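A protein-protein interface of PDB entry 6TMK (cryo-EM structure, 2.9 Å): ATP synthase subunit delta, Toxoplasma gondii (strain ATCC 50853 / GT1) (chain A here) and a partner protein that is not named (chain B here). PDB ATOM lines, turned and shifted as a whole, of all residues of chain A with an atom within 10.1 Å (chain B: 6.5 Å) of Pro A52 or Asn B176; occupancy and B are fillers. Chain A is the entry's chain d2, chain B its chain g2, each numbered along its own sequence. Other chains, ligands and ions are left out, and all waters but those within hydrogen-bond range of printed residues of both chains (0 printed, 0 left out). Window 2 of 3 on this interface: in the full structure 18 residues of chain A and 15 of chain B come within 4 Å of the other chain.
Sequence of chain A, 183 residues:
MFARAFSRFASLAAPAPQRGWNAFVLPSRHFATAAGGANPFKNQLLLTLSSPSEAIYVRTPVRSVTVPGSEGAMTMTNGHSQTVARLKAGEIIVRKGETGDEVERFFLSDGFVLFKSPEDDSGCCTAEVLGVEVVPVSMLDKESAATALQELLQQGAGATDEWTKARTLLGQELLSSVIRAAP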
ATOM      1  N   LEU A  49       4.400  -7.511 -20.082  1.00  0.00           N
ATOM      2  CA  LEU A  49       4.247  -6.710 -21.288  1.00  0.00           C
ATOM      3  C   LEU A  49       5.643  -6.400 -21.804  1.00  0.00           C
ATOM      4  O   LEU A  49       6.414  -5.708 -21.132  1.00  0.00           O
ATOM      5  CB  LEU A  49       3.477  -5.423 -20.998  1.00  0.00           C
ATOM      6  CG  LEU A  49       3.332  -4.434 -22.156  1.00  0.00           C
ATOM      7  CD1 LEU A  49       2.568  -5.046 -23.310  1.00  0.00           C
ATOM      8  CD2 LEU A  49       2.652  -3.169 -21.675  1.00  0.00           C
ATOM      9  N   SER A  50       5.966  -6.906 -22.992  1.00  0.00           N
ATOM     10  CA  SER A  50       7.354  -6.962 -23.420  1.00  0.00           C
ATOM     11  C   SER A  50       7.486  -6.613 -24.892  1.00  0.00           C
ATOM     12  O   SER A  50       6.703  -7.070 -25.729  1.00  0.00           O
ATOM     13  CB  SER A  50       7.947  -8.353 -23.174  1.00  0.00           C
ATOM     14  OG  SER A  50       7.681  -8.792 -21.854  1.00  0.00           O
ATOM     15  N   SER A  51       8.484  -5.798 -25.188  1.00  0.00           N
ATOM     16  CA  SER A  51       9.026  -5.587 -26.514  1.00  0.00           C
ATOM     17  C   SER A  51      10.436  -6.151 -26.583  1.00  0.00           C
ATOM     18  O   SER A  51      11.018  -6.534 -25.563  1.00  0.00           O
ATOM     19  CB  SER A  51       9.038  -4.092 -26.851  1.00  0.00           C
ATOM     20  OG  SER A  51       9.908  -3.383 -25.988  1.00  0.00           O
ATOM     21  N   PRO A  52      11.023  -6.225 -27.780  1.00  0.00           N
ATOM     22  CA  PRO A  52      12.396  -6.743 -27.860  1.00  0.00           C
ATOM     23  C   PRO A  52      13.398  -5.848 -27.158  1.00  0.00           C
ATOM     24  O   PRO A  52      14.348  -6.349 -26.543  1.00  0.00           O
ATOM     25  CB  PRO A  52      12.654  -6.822 -29.372  1.00  0.00           C
ATOM     26  CG  PRO A  52      11.301  -6.820 -29.997  1.00  0.00           C
ATOM     27  CD  PRO A  52      10.465  -5.957 -29.113  1.00  0.00           C
ATOM     28  N   SER A  53      13.213  -4.531 -27.232  1.00  0.00           N
ATOM     29  CA  SER A  53      14.189  -3.590 -26.703  1.00  0.00           C
ATOM     30  C   SER A  53      14.001  -3.298 -25.221  1.00  0.00           C
ATOM     31  O   SER A  53      14.924  -2.773 -24.588  1.00  0.00           O
ATOM     32  CB  SER A  53      14.122  -2.275 -27.484  1.00  0.00           C
ATOM     33  OG  SER A  53      14.117  -2.515 -28.881  1.00  0.00           O
ATOM     34  N   GLU A  54      12.839  -3.619 -24.654  1.00  0.00           N
ATOM     35  CA  GLU A  54      12.565  -3.283 -23.263  1.00  0.00           C
ATOM     36  C   GLU A  54      11.406  -4.128 -22.758  1.00  0.00           C
ATOM     37  O   GLU A  54      10.360  -4.201 -23.411  1.00  0.00           O
ATOM     38  CB  GLU A  54      12.238  -1.793 -23.115  1.00  0.00           C
ATOM     39  CG  GLU A  54      12.318  -1.279 -21.688  1.00  0.00           C
ATOM     40  CD  GLU A  54      11.798   0.137 -21.547  1.00  0.00           C
ATOM     41  OE1 GLU A  54      11.200   0.652 -22.515  1.00  0.00           O
ATOM     42  OE2 GLU A  54      11.987   0.737 -20.467  1.00  0.00           O
ATOM     43  N   ALA A  55      11.596  -4.758 -21.601  1.00  0.00           N
ATOM     44  CA  ALA A  55      10.533  -5.466 -20.896  1.00  0.00           C
ATOM     45  C   ALA A  55       9.954  -4.528 -19.842  1.00  0.00           C
ATOM     46  O   ALA A  55      10.613  -4.229 -18.841  1.00  0.00           O
ATOM     47  CB  ALA A  55      11.063  -6.749 -20.260  1.00  0.00           C
ATOM     48  N   ILE A  56       8.725  -4.066 -20.067  1.00  0.00           N
ATOM     49  CA  ILE A  56       8.120  -3.110 -19.147  1.00  0.00           C
ATOM     50  C   ILE A  56       7.597  -3.809 -17.899  1.00  0.00           C
ATOM     51  O   ILE A  56       7.665  -3.259 -16.794  1.00  0.00           O
ATOM     52  CB  ILE A  56       7.007  -2.327 -19.862  1.00  0.00           C
ATOM     53  CG1 ILE A  56       7.607  -1.409 -20.926  1.00  0.00           C
ATOM     54  CG2 ILE A  56       6.200  -1.522 -18.860  1.00  0.00           C
ATOM     55  CD1 ILE A  56       6.683  -1.135 -22.085  1.00  0.00           C
ATOM     56  N   LEU A 108       0.772  -0.024 -28.791  1.00  0.00           N
ATOM     57  CA  LEU A 108       1.371  -1.191 -29.416  1.00  0.00           C
ATOM     58  C   LEU A 108       1.135  -1.136 -30.917  1.00  0.00           C
ATOM     59  O   LEU A 108       0.040  -0.787 -31.371  1.00  0.00           O
ATOM     60  CB  LEU A 108       0.787  -2.483 -28.846  1.00  0.00           C
ATOM     61  CG  LEU A 108       1.420  -3.773 -29.362  1.00  0.00           C
ATOM     62  CD1 LEU A 108       1.668  -4.752 -28.232  1.00  0.00           C
ATOM     63  CD2 LEU A 108       0.529  -4.396 -30.417  1.00  0.00           C
ATOM     64  N   SER A 109       2.165  -1.486 -31.685  1.00  0.00           N
ATOM     65  CA  SER A 109       2.032  -1.535 -33.137  1.00  0.00           C
ATOM     66  C   SER A 109       1.419  -2.857 -33.580  1.00  0.00           C
ATOM     67  O   SER A 109       0.318  -2.891 -34.138  1.00  0.00           O
ATOM     68  CB  SER A 109       3.395  -1.328 -33.797  1.00  0.00           C
ATOM     69  OG  SER A 109       3.368  -1.732 -35.154  1.00  0.00           O
ATOM     70  N   ASP A 110       2.120  -3.958 -33.324  1.00  0.00           N
ATOM     71  CA  ASP A 110       1.712  -5.271 -33.795  1.00  0.00           C
ATOM     72  C   ASP A 110       2.307  -6.316 -32.866  1.00  0.00           C
ATOM     73  O   ASP A 110       3.312  -6.074 -32.192  1.00  0.00           O
ATOM     74  CB  ASP A 110       2.162  -5.516 -35.238  1.00  0.00           C
ATOM     75  CG  ASP A 110       1.349  -4.730 -36.245  1.00  0.00           C
ATOM     76  OD1 ASP A 110       0.127  -4.574 -36.036  1.00  0.00           O
ATOM     77  OD2 ASP A 110       1.933  -4.255 -37.241  1.00  0.00           O
ATOM     78  N   GLY A 111       1.685  -7.476 -32.839  1.00  0.00           N
ATOM     79  CA  GLY A 111       2.199  -8.573 -32.048  1.00  0.00           C
ATOM     80  C   GLY A 111       1.076  -9.510 -31.643  1.00  0.00           C
ATOM     81  O   GLY A 111       0.069  -9.626 -32.339  1.00  0.00           O
ATOM     82  N   VAL A 129       1.930 -10.167 -23.181  1.00  0.00           N
ATOM     83  CA  VAL A 129       1.593  -9.236 -24.250  1.00  0.00           C
ATOM     84  C   VAL A 129       2.888  -8.860 -24.956  1.00  0.00           C
ATOM     85  O   VAL A 129       3.695  -8.081 -24.428  1.00  0.00           O
ATOM     86  CB  VAL A 129       0.869  -7.994 -23.717  1.00  0.00           C
ATOM     87  CG1 VAL A 129       0.538  -7.052 -24.855  1.00  0.00           C
ATOM     88  CG2 VAL A 129      -0.392  -8.396 -22.984  1.00  0.00           C
ATOM     89  N   LEU A 130       3.079  -9.397 -26.158  1.00  0.00           N
ATOM     90  CA  LEU A 130       4.302  -9.207 -26.923  1.00  0.00           C
ATOM     91  C   LEU A 130       4.056  -8.199 -28.035  1.00  0.00           C
ATOM     92  O   LEU A 130       3.111  -8.343 -28.816  1.00  0.00           O
ATOM     93  CB  LEU A 130       4.786 -10.531 -27.515  1.00  0.00           C
ATOM     94  CG  LEU A 130       4.658 -11.753 -26.608  1.00  0.00           C
ATOM     95  CD1 LEU A 130       5.050 -13.011 -27.359  1.00  0.00           C
ATOM     96  CD2 LEU A 130       5.508 -11.574 -25.366  1.00  0.00           C
ATOM     97  N   GLY A 131       4.902  -7.187 -28.095  1.00  0.00           N
ATOM     98  CA  GLY A 131       4.768  -6.134 -29.087  1.00  0.00           C
ATOM     99  C   GLY A 131       6.089  -5.842 -29.760  1.00  0.00           C
ATOM    100  O   GLY A 131       7.128  -5.771 -29.108  1.00  0.00           O
ATOM    101  N   VAL A 132       6.037  -5.675 -31.083  1.00  0.00           N
ATOM    102  CA  VAL A 132       7.250  -5.394 -31.838  1.00  0.00           C
ATOM    103  C   VAL A 132       7.776  -4.001 -31.530  1.00  0.00           C
ATOM    104  O   VAL A 132       8.975  -3.742 -31.691  1.00  0.00           O
ATOM    105  CB  VAL A 132       6.989  -5.560 -33.346  1.00  0.00           C
ATOM    106  CG1 VAL A 132       8.280  -5.417 -34.131  1.00  0.00           C
ATOM    107  CG2 VAL A 132       6.354  -6.910 -33.619  1.00  0.00           C
ATOM    108  N   GLU A 133       6.907  -3.094 -31.089  1.00  0.00           N
ATOM    109  CA  GLU A 133       7.335  -1.768 -30.651  1.00  0.00           C
ATOM    110  C   GLU A 133       6.273  -1.250 -29.693  1.00  0.00           C
ATOM    111  O   GLU A 133       5.175  -0.886 -30.127  1.00  0.00           O
ATOM    112  CB  GLU A 133       7.519  -0.830 -31.835  1.00  0.00           C
ATOM    113  CG  GLU A 133       8.300   0.428 -31.503  1.00  0.00           C
ATOM    114  CD  GLU A 133       9.790   0.177 -31.385  1.00  0.00           C
ATOM    115  OE1 GLU A 133      10.433  -0.094 -32.420  1.00  0.00           O
ATOM    116  OE2 GLU A 133      10.318   0.251 -30.254  1.00  0.00           O
ATOM    117  N   VAL A 134       6.598  -1.220 -28.406  1.00  0.00           N
ATOM    118  CA  VAL A 134       5.668  -0.808 -27.362  1.00  0.00           C
ATOM    119  C   VAL A 134       6.179   0.491 -26.757  1.00  0.00           C
ATOM    120  O   VAL A 134       7.190   0.499 -26.044  1.00  0.00           O
ATOM    121  CB  VAL A 134       5.510  -1.891 -26.287  1.00  0.00           C
ATOM    122  CG1 VAL A 134       4.826  -1.321 -25.059  1.00  0.00           C
ATOM    123  CG2 VAL A 134       4.735  -3.067 -26.839  1.00  0.00           C
ATOM    124  N   VAL A 135       5.484   1.586 -27.038  1.00  0.00           N
ATOM    125  CA  VAL A 135       5.828   2.888 -26.473  1.00  0.00           C
ATOM    126  C   VAL A 135       4.775   3.228 -25.426  1.00  0.00           C
ATOM    127  O   VAL A 135       3.663   2.682 -25.473  1.00  0.00           O
ATOM    128  CB  VAL A 135       5.906   3.969 -27.561  1.00  0.00           C
ATOM    129  CG1 VAL A 135       6.548   5.232 -27.016  1.00  0.00           C
ATOM    130  CG2 VAL A 135       6.675   3.456 -28.760  1.00  0.00           C
ATOM    131  N   ARG B  77      20.788  -6.878 -22.603  1.00  0.00           N
ATOM    132  CA  ARG B  77      19.936  -7.114 -23.766  1.00  0.00           C
ATOM    133  C   ARG B  77      19.272  -8.484 -23.694  1.00  0.00           C
ATOM    134  O   ARG B  77      18.107  -8.638 -24.073  1.00  0.00           O
ATOM    135  CB  ARG B  77      20.751  -6.983 -25.050  1.00  0.00           C
ATOM    136  CG  ARG B  77      21.193  -5.565 -25.358  1.00  0.00           C
ATOM    137  CD  ARG B  77      21.840  -5.472 -26.729  1.00  0.00           C
ATOM    138  NE  ARG B  77      22.645  -4.263 -26.874  1.00  0.00           N
ATOM    139  CZ  ARG B  77      23.848  -4.094 -26.335  1.00  0.00           C
ATOM    140  NH1 ARG B  77      24.406  -5.060 -25.616  1.00  0.00           N
ATOM    141  NH2 ARG B  77      24.503  -2.957 -26.522  1.00  0.00           N
ATOM    142  N   ASN B  80      16.428  -8.453 -21.155  1.00  0.00           N
ATOM    143  CA  ASN B  80      15.292  -7.675 -21.635  1.00  0.00           C
ATOM    144  C   ASN B  80      14.577  -8.349 -22.805  1.00  0.00           C
ATOM    145  O   ASN B  80      13.360  -8.188 -22.948  1.00  0.00           O
ATOM    146  CB  ASN B  80      15.744  -6.272 -22.041  1.00  0.00           C
ATOM    147  CG  ASN B  80      16.194  -5.441 -20.857  1.00  0.00           C
ATOM    148  OD1 ASN B  80      15.589  -5.489 -19.787  1.00  0.00           O
ATOM    149  ND2 ASN B  80      17.254  -4.667 -21.047  1.00  0.00           N
ATOM    150  N   GLY B  81      15.295  -9.100 -23.639  1.00  0.00           N
ATOM    151  CA  GLY B  81      14.746  -9.582 -24.891  1.00  0.00           C
ATOM    152  C   GLY B  81      14.382 -11.054 -24.927  1.00  0.00           C
ATOM    153  O   GLY B  81      13.844 -11.533 -25.930  1.00  0.00           O
ATOM    154  N   LEU B  82      14.666 -11.785 -23.854  1.00  0.00           N
ATOM    155  CA  LEU B  82      14.314 -13.199 -23.778  1.00  0.00           C
ATOM    156  C   LEU B  82      12.838 -13.416 -23.456  1.00  0.00           C
ATOM    157  O   LEU B  82      12.182 -14.248 -24.095  1.00  0.00           O
ATOM    158  CB  LEU B  82      15.174 -13.903 -22.727  1.00  0.00           C
ATOM    159  CG  LEU B  82      16.494 -14.529 -23.178  1.00  0.00           C
ATOM    160  CD1 LEU B  82      17.139 -15.253 -22.010  1.00  0.00           C
ATOM    161  CD2 LEU B  82      16.297 -15.480 -24.349  1.00  0.00           C
ATOM    162  N   PHE B  84      10.426 -11.773 -24.415  1.00  0.00           N
ATOM    163  CA  PHE B  84       9.694 -11.599 -25.663  1.00  0.00           C
ATOM    164  C   PHE B  84       9.617 -12.873 -26.499  1.00  0.00           C
ATOM    165  O   PHE B  84       8.718 -12.987 -27.341  1.00  0.00           O
ATOM    166  CB  PHE B  84      10.361 -10.485 -26.472  1.00  0.00           C
ATOM    167  CG  PHE B  84       9.678 -10.173 -27.767  1.00  0.00           C
ATOM    168  CD1 PHE B  84       8.566  -9.352 -27.796  1.00  0.00           C
ATOM    169  CD2 PHE B  84      10.155 -10.688 -28.956  1.00  0.00           C
ATOM    170  CE1 PHE B  84       7.939  -9.057 -28.989  1.00  0.00           C
ATOM    171  CE2 PHE B  84       9.533 -10.398 -30.150  1.00  0.00           C
ATOM    172  CZ  PHE B  84       8.424  -9.580 -30.165  1.00  0.00           C
ATOM    173  N   PRO B 174      24.687  -3.390 -32.012  1.00  0.00           N
ATOM    174  CA  PRO B 174      23.925  -4.403 -31.272  1.00  0.00           C
ATOM    175  C   PRO B 174      23.037  -5.244 -32.174  1.00  0.00           C
ATOM    176  O   PRO B 174      22.998  -5.045 -33.392  1.00  0.00           O
ATOM    177  CB  PRO B 174      23.094  -3.566 -30.297  1.00  0.00           C
ATOM    178  CG  PRO B 174      23.911  -2.343 -30.049  1.00  0.00           C
ATOM    179  CD  PRO B 174      24.834  -2.146 -31.237  1.00  0.00           C
ATOM    180  N   TRP B 175      22.319  -6.195 -31.577  1.00  0.00           N
ATOM    181  CA  TRP B 175      21.809  -7.343 -32.318  1.00  0.00           C
ATOM    182  C   TRP B 175      20.615  -6.980 -33.192  1.00  0.00           C
ATOM    183  O   TRP B 175      20.681  -7.086 -34.421  1.00  0.00           O
ATOM    184  CB  TRP B 175      21.448  -8.463 -31.341  1.00  0.00           C
ATOM    185  CG  TRP B 175      20.635  -9.564 -31.939  1.00  0.00           C
ATOM    186  CD1 TRP B 175      19.597 -10.218 -31.352  1.00  0.00           C
ATOM    187  CD2 TRP B 175      20.788 -10.141 -33.242  1.00  0.00           C
ATOM    188  NE1 TRP B 175      19.094 -11.169 -32.203  1.00  0.00           N
ATOM    189  CE2 TRP B 175      19.806 -11.140 -33.372  1.00  0.00           C
ATOM    190  CE3 TRP B 175      21.656  -9.907 -34.312  1.00  0.00           C
ATOM    191  CZ2 TRP B 175      19.669 -11.907 -34.525  1.00  0.00           C
ATOM    192  CZ3 TRP B 175      21.517 -10.669 -35.455  1.00  0.00           C
ATOM    193  CH2 TRP B 175      20.532 -11.656 -35.552  1.00  0.00           C
ATOM    194  N   ASN B 176      19.516  -6.549 -32.587  1.00  0.00           N
ATOM    195  CA  ASN B 176      18.296  -6.417 -33.385  1.00  0.00           C
ATOM    196  C   ASN B 176      18.352  -5.260 -34.348  1.00  0.00           C
ATOM    197  O   ASN B 176      17.345  -4.971 -35.005  1.00  0.00           O
ATOM    198  CB  ASN B 176      17.083  -6.257 -32.469  1.00  0.00           C
ATOM    199  CG  ASN B 176      15.832  -6.895 -33.040  1.00  0.00           C
ATOM    200  OD1 ASN B 176      15.896  -7.704 -33.966  1.00  0.00           O
ATOM    201  ND2 ASN B 176      14.682  -6.528 -32.489  1.00  0.00           N
ATOM    202  N   PHE B 177      19.498  -4.590 -34.444  1.00  0.00           N
ATOM    203  CA  PHE B 177      19.852  -3.843 -35.642  1.00  0.00           C
ATOM    204  C   PHE B 177      19.586  -4.696 -36.875  1.00  0.00           C
ATOM    205  O   PHE B 177      18.716  -4.378 -37.692  1.00  0.00           O
ATOM    206  CB  PHE B 177      21.323  -3.430 -35.601  1.00  0.00           C
ATOM    207  CG  PHE B 177      21.598  -2.251 -34.718  1.00  0.00           C
ATOM    208  CD1 PHE B 177      21.688  -2.407 -33.346  1.00  0.00           C
ATOM    209  CD2 PHE B 177      21.800  -0.995 -35.258  1.00  0.00           C
ATOM    210  CE1 PHE B 177      21.949  -1.329 -32.529  1.00  0.00           C
ATOM    211  CE2 PHE B 177      22.073   0.085 -34.443  1.00  0.00           C
ATOM    212  CZ  PHE B 177      22.139  -0.082 -33.076  1.00  0.00           C
ATOM    213  N   GLY B 178      20.339  -5.786 -37.006  1.00  0.00           N
ATOM    214  CA  GLY B 178      20.167  -6.741 -38.083  1.00  0.00           C
ATOM    215  C   GLY B 178      19.037  -7.709 -37.805  1.00  0.00           C
ATOM    216  O   GLY B 178      19.274  -8.865 -37.446  1.00  0.00           O
ATOM    217  N   GLN B 179      17.802  -7.242 -37.972  1.00  0.00           N
ATOM    218  CA  GLN B 179      16.654  -7.930 -37.401  1.00  0.00           C
ATOM    219  C   GLN B 179      16.586  -9.381 -37.856  1.00  0.00           C
ATOM    220  O   GLN B 179      16.847  -9.707 -39.017  1.00  0.00           O
ATOM    221  CB  GLN B 179      15.361  -7.208 -37.776  1.00  0.00           C
ATOM    222  CG  GLN B 179      15.228  -5.832 -37.166  1.00  0.00           C
ATOM    223  CD  GLN B 179      13.917  -5.163 -37.522  1.00  0.00           C
ATOM    224  OE1 GLN B 179      13.095  -5.730 -38.241  1.00  0.00           O
ATOM    225  NE2 GLN B 179      13.716  -3.952 -37.020  1.00  0.00           N
ATOM    226  N   ALA B 180      16.237 -10.253 -36.909  1.00  0.00           N
ATOM    227  CA  ALA B 180      15.993 -11.659 -37.198  1.00  0.00           C
ATOM    228  C   ALA B 180      14.839 -11.848 -38.169  1.00  0.00           C
ATOM    229  O   ALA B 180      14.754 -12.897 -38.816  1.00  0.00           O
ATOM    230  CB  ALA B 180      15.717 -12.413 -35.901  1.00  0.00           C
ATOM    231  N   CYS B 181      13.932 -10.873 -38.251  1.00  0.00           N
ATOM    232  CA  CYS B 181      12.800 -10.976 -39.165  1.00  0.00           C
ATOM    233  C   CYS B 181      13.269 -11.135 -40.604  1.00  0.00           C
ATOM    234  O   CYS B 181      12.654 -11.866 -41.387  1.00  0.00           O
ATOM    235  CB  CYS B 181      11.907  -9.745 -39.030  1.00  0.00           C
ATOM    236  SG  CYS B 181      10.947  -9.675 -37.500  1.00  0.00           S
ATOM    237  N   PHE B 255      16.130 -14.796 -32.637  1.00  0.00           N
ATOM    238  CA  PHE B 255      16.502 -13.678 -31.776  1.00  0.00           C
ATOM    239  C   PHE B 255      17.201 -14.156 -30.504  1.00  0.00           C
ATOM    240  O   PHE B 255      18.348 -13.776 -30.221  1.00  0.00           O
ATOM    241  CB  PHE B 255      15.236 -12.883 -31.449  1.00  0.00           C
ATOM    242  CG  PHE B 255      15.471 -11.633 -30.658  1.00  0.00           C
ATOM    243  CD1 PHE B 255      16.219 -10.598 -31.181  1.00  0.00           C
ATOM    244  CD2 PHE B 255      14.908 -11.480 -29.405  1.00  0.00           C
ATOM    245  CE1 PHE B 255      16.422  -9.439 -30.460  1.00  0.00           C
ATOM    246  CE2 PHE B 255      15.106 -10.326 -28.679  1.00  0.00           C
ATOM    247  CZ  PHE B 255      15.865  -9.303 -29.207  1.00  0.00           C
ATOM    248  N   LEU B 259      21.207 -13.899 -29.329  1.00  0.00           N
ATOM    249  CA  LEU B 259      21.595 -13.222 -28.094  1.00  0.00           C
ATOM    250  C   LEU B 259      22.478 -14.125 -27.237  1.00  0.00           C
ATOM    251  O   LEU B 259      23.534 -13.705 -26.735  1.00  0.00           O
ATOM    252  CB  LEU B 259      20.353 -12.793 -27.319  1.00  0.00           C
ATOM    253  CG  LEU B 259      19.498 -11.717 -27.982  1.00  0.00           C
ATOM    254  CD1 LEU B 259      18.124 -11.685 -27.353  1.00  0.00           C
ATOM    255  CD2 LEU B 259      20.169 -10.366 -27.872  1.00  0.00           C
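Of the printed residues of chain B, Ser A50 touches Phe B84 (3.6 Å).
Printed residues of chain B within 4 Å of Ser A51: Asn B80 and Phe B84.
Printed residues of chain B within 4 Å of Pro A52: Gly B81 (3.7 Å), Phe B84 (3.98 Å) and Asn B176 (3.7 Å).
Leu A108 touches none of the printed residues of chain B.
Of the printed residues of chain B, Leu A130 touches Phe B84 (3.7 Å).
Printed residues of chain A within 4 Å of Asn B80: Ser A51 and Ala A55.
Of chain A, only Pro A52 (3.7 Å) comes within 4 Å of Gly B81.
Printed residues of chain A within 4 Å of Phe B84: Ser A50, Ser A51, Pro A52, Leu A130 and Gly A131.
Trp B175 touches none of the printed residues of chain A.
Printed residues of chain A within 4 Å of Asn B176: Pro A52.
No residue of chain A comes within 4 Å of Gly B178.
No residue of chain A comes within 4 Å of Gln B179.
Hydrophobic or aromatic side chains of chain B within 4 Å of the printed part of chain A: Phe B84.
Hydrophobic or aromatic side chains of chain A that line the printed part of chain B: Pro A52, Ala A55 and Leu A130.
Among the printed residues, no Asp or Glu carboxylate lies within 4 Å of a Lys or Arg side-chain nitrogen of the other chain.
The backbone NH of Ser A50 lies within hydrogen-bond range of the backbone carbonyl oxygen of Val A129, at 2.9 Å.
The backbone carbonyl oxygen (O) of Ser A50 is in hydrogen-bond range of the backbone NH (N) of Gly A131 (3.0 Å).
The side-chain hydroxyl (OG) of Ser A51 sits at hydrogen-bond distance from the backbone carbonyl oxygen (O) of Glu A54, 2.7 Å away.
Among the printed residues, merely in contact across the chains: Gly A131 with Phe B84, Ser A50 with Phe B84, Pro A52 with Gly B81, Leu A130 with Phe B84, Pro A52 with Asn B176, Ala A55 with Asn B80, Ser A51 with Asn B80, Ser A51 with Phe B84 and Pro A52 with Phe B84.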
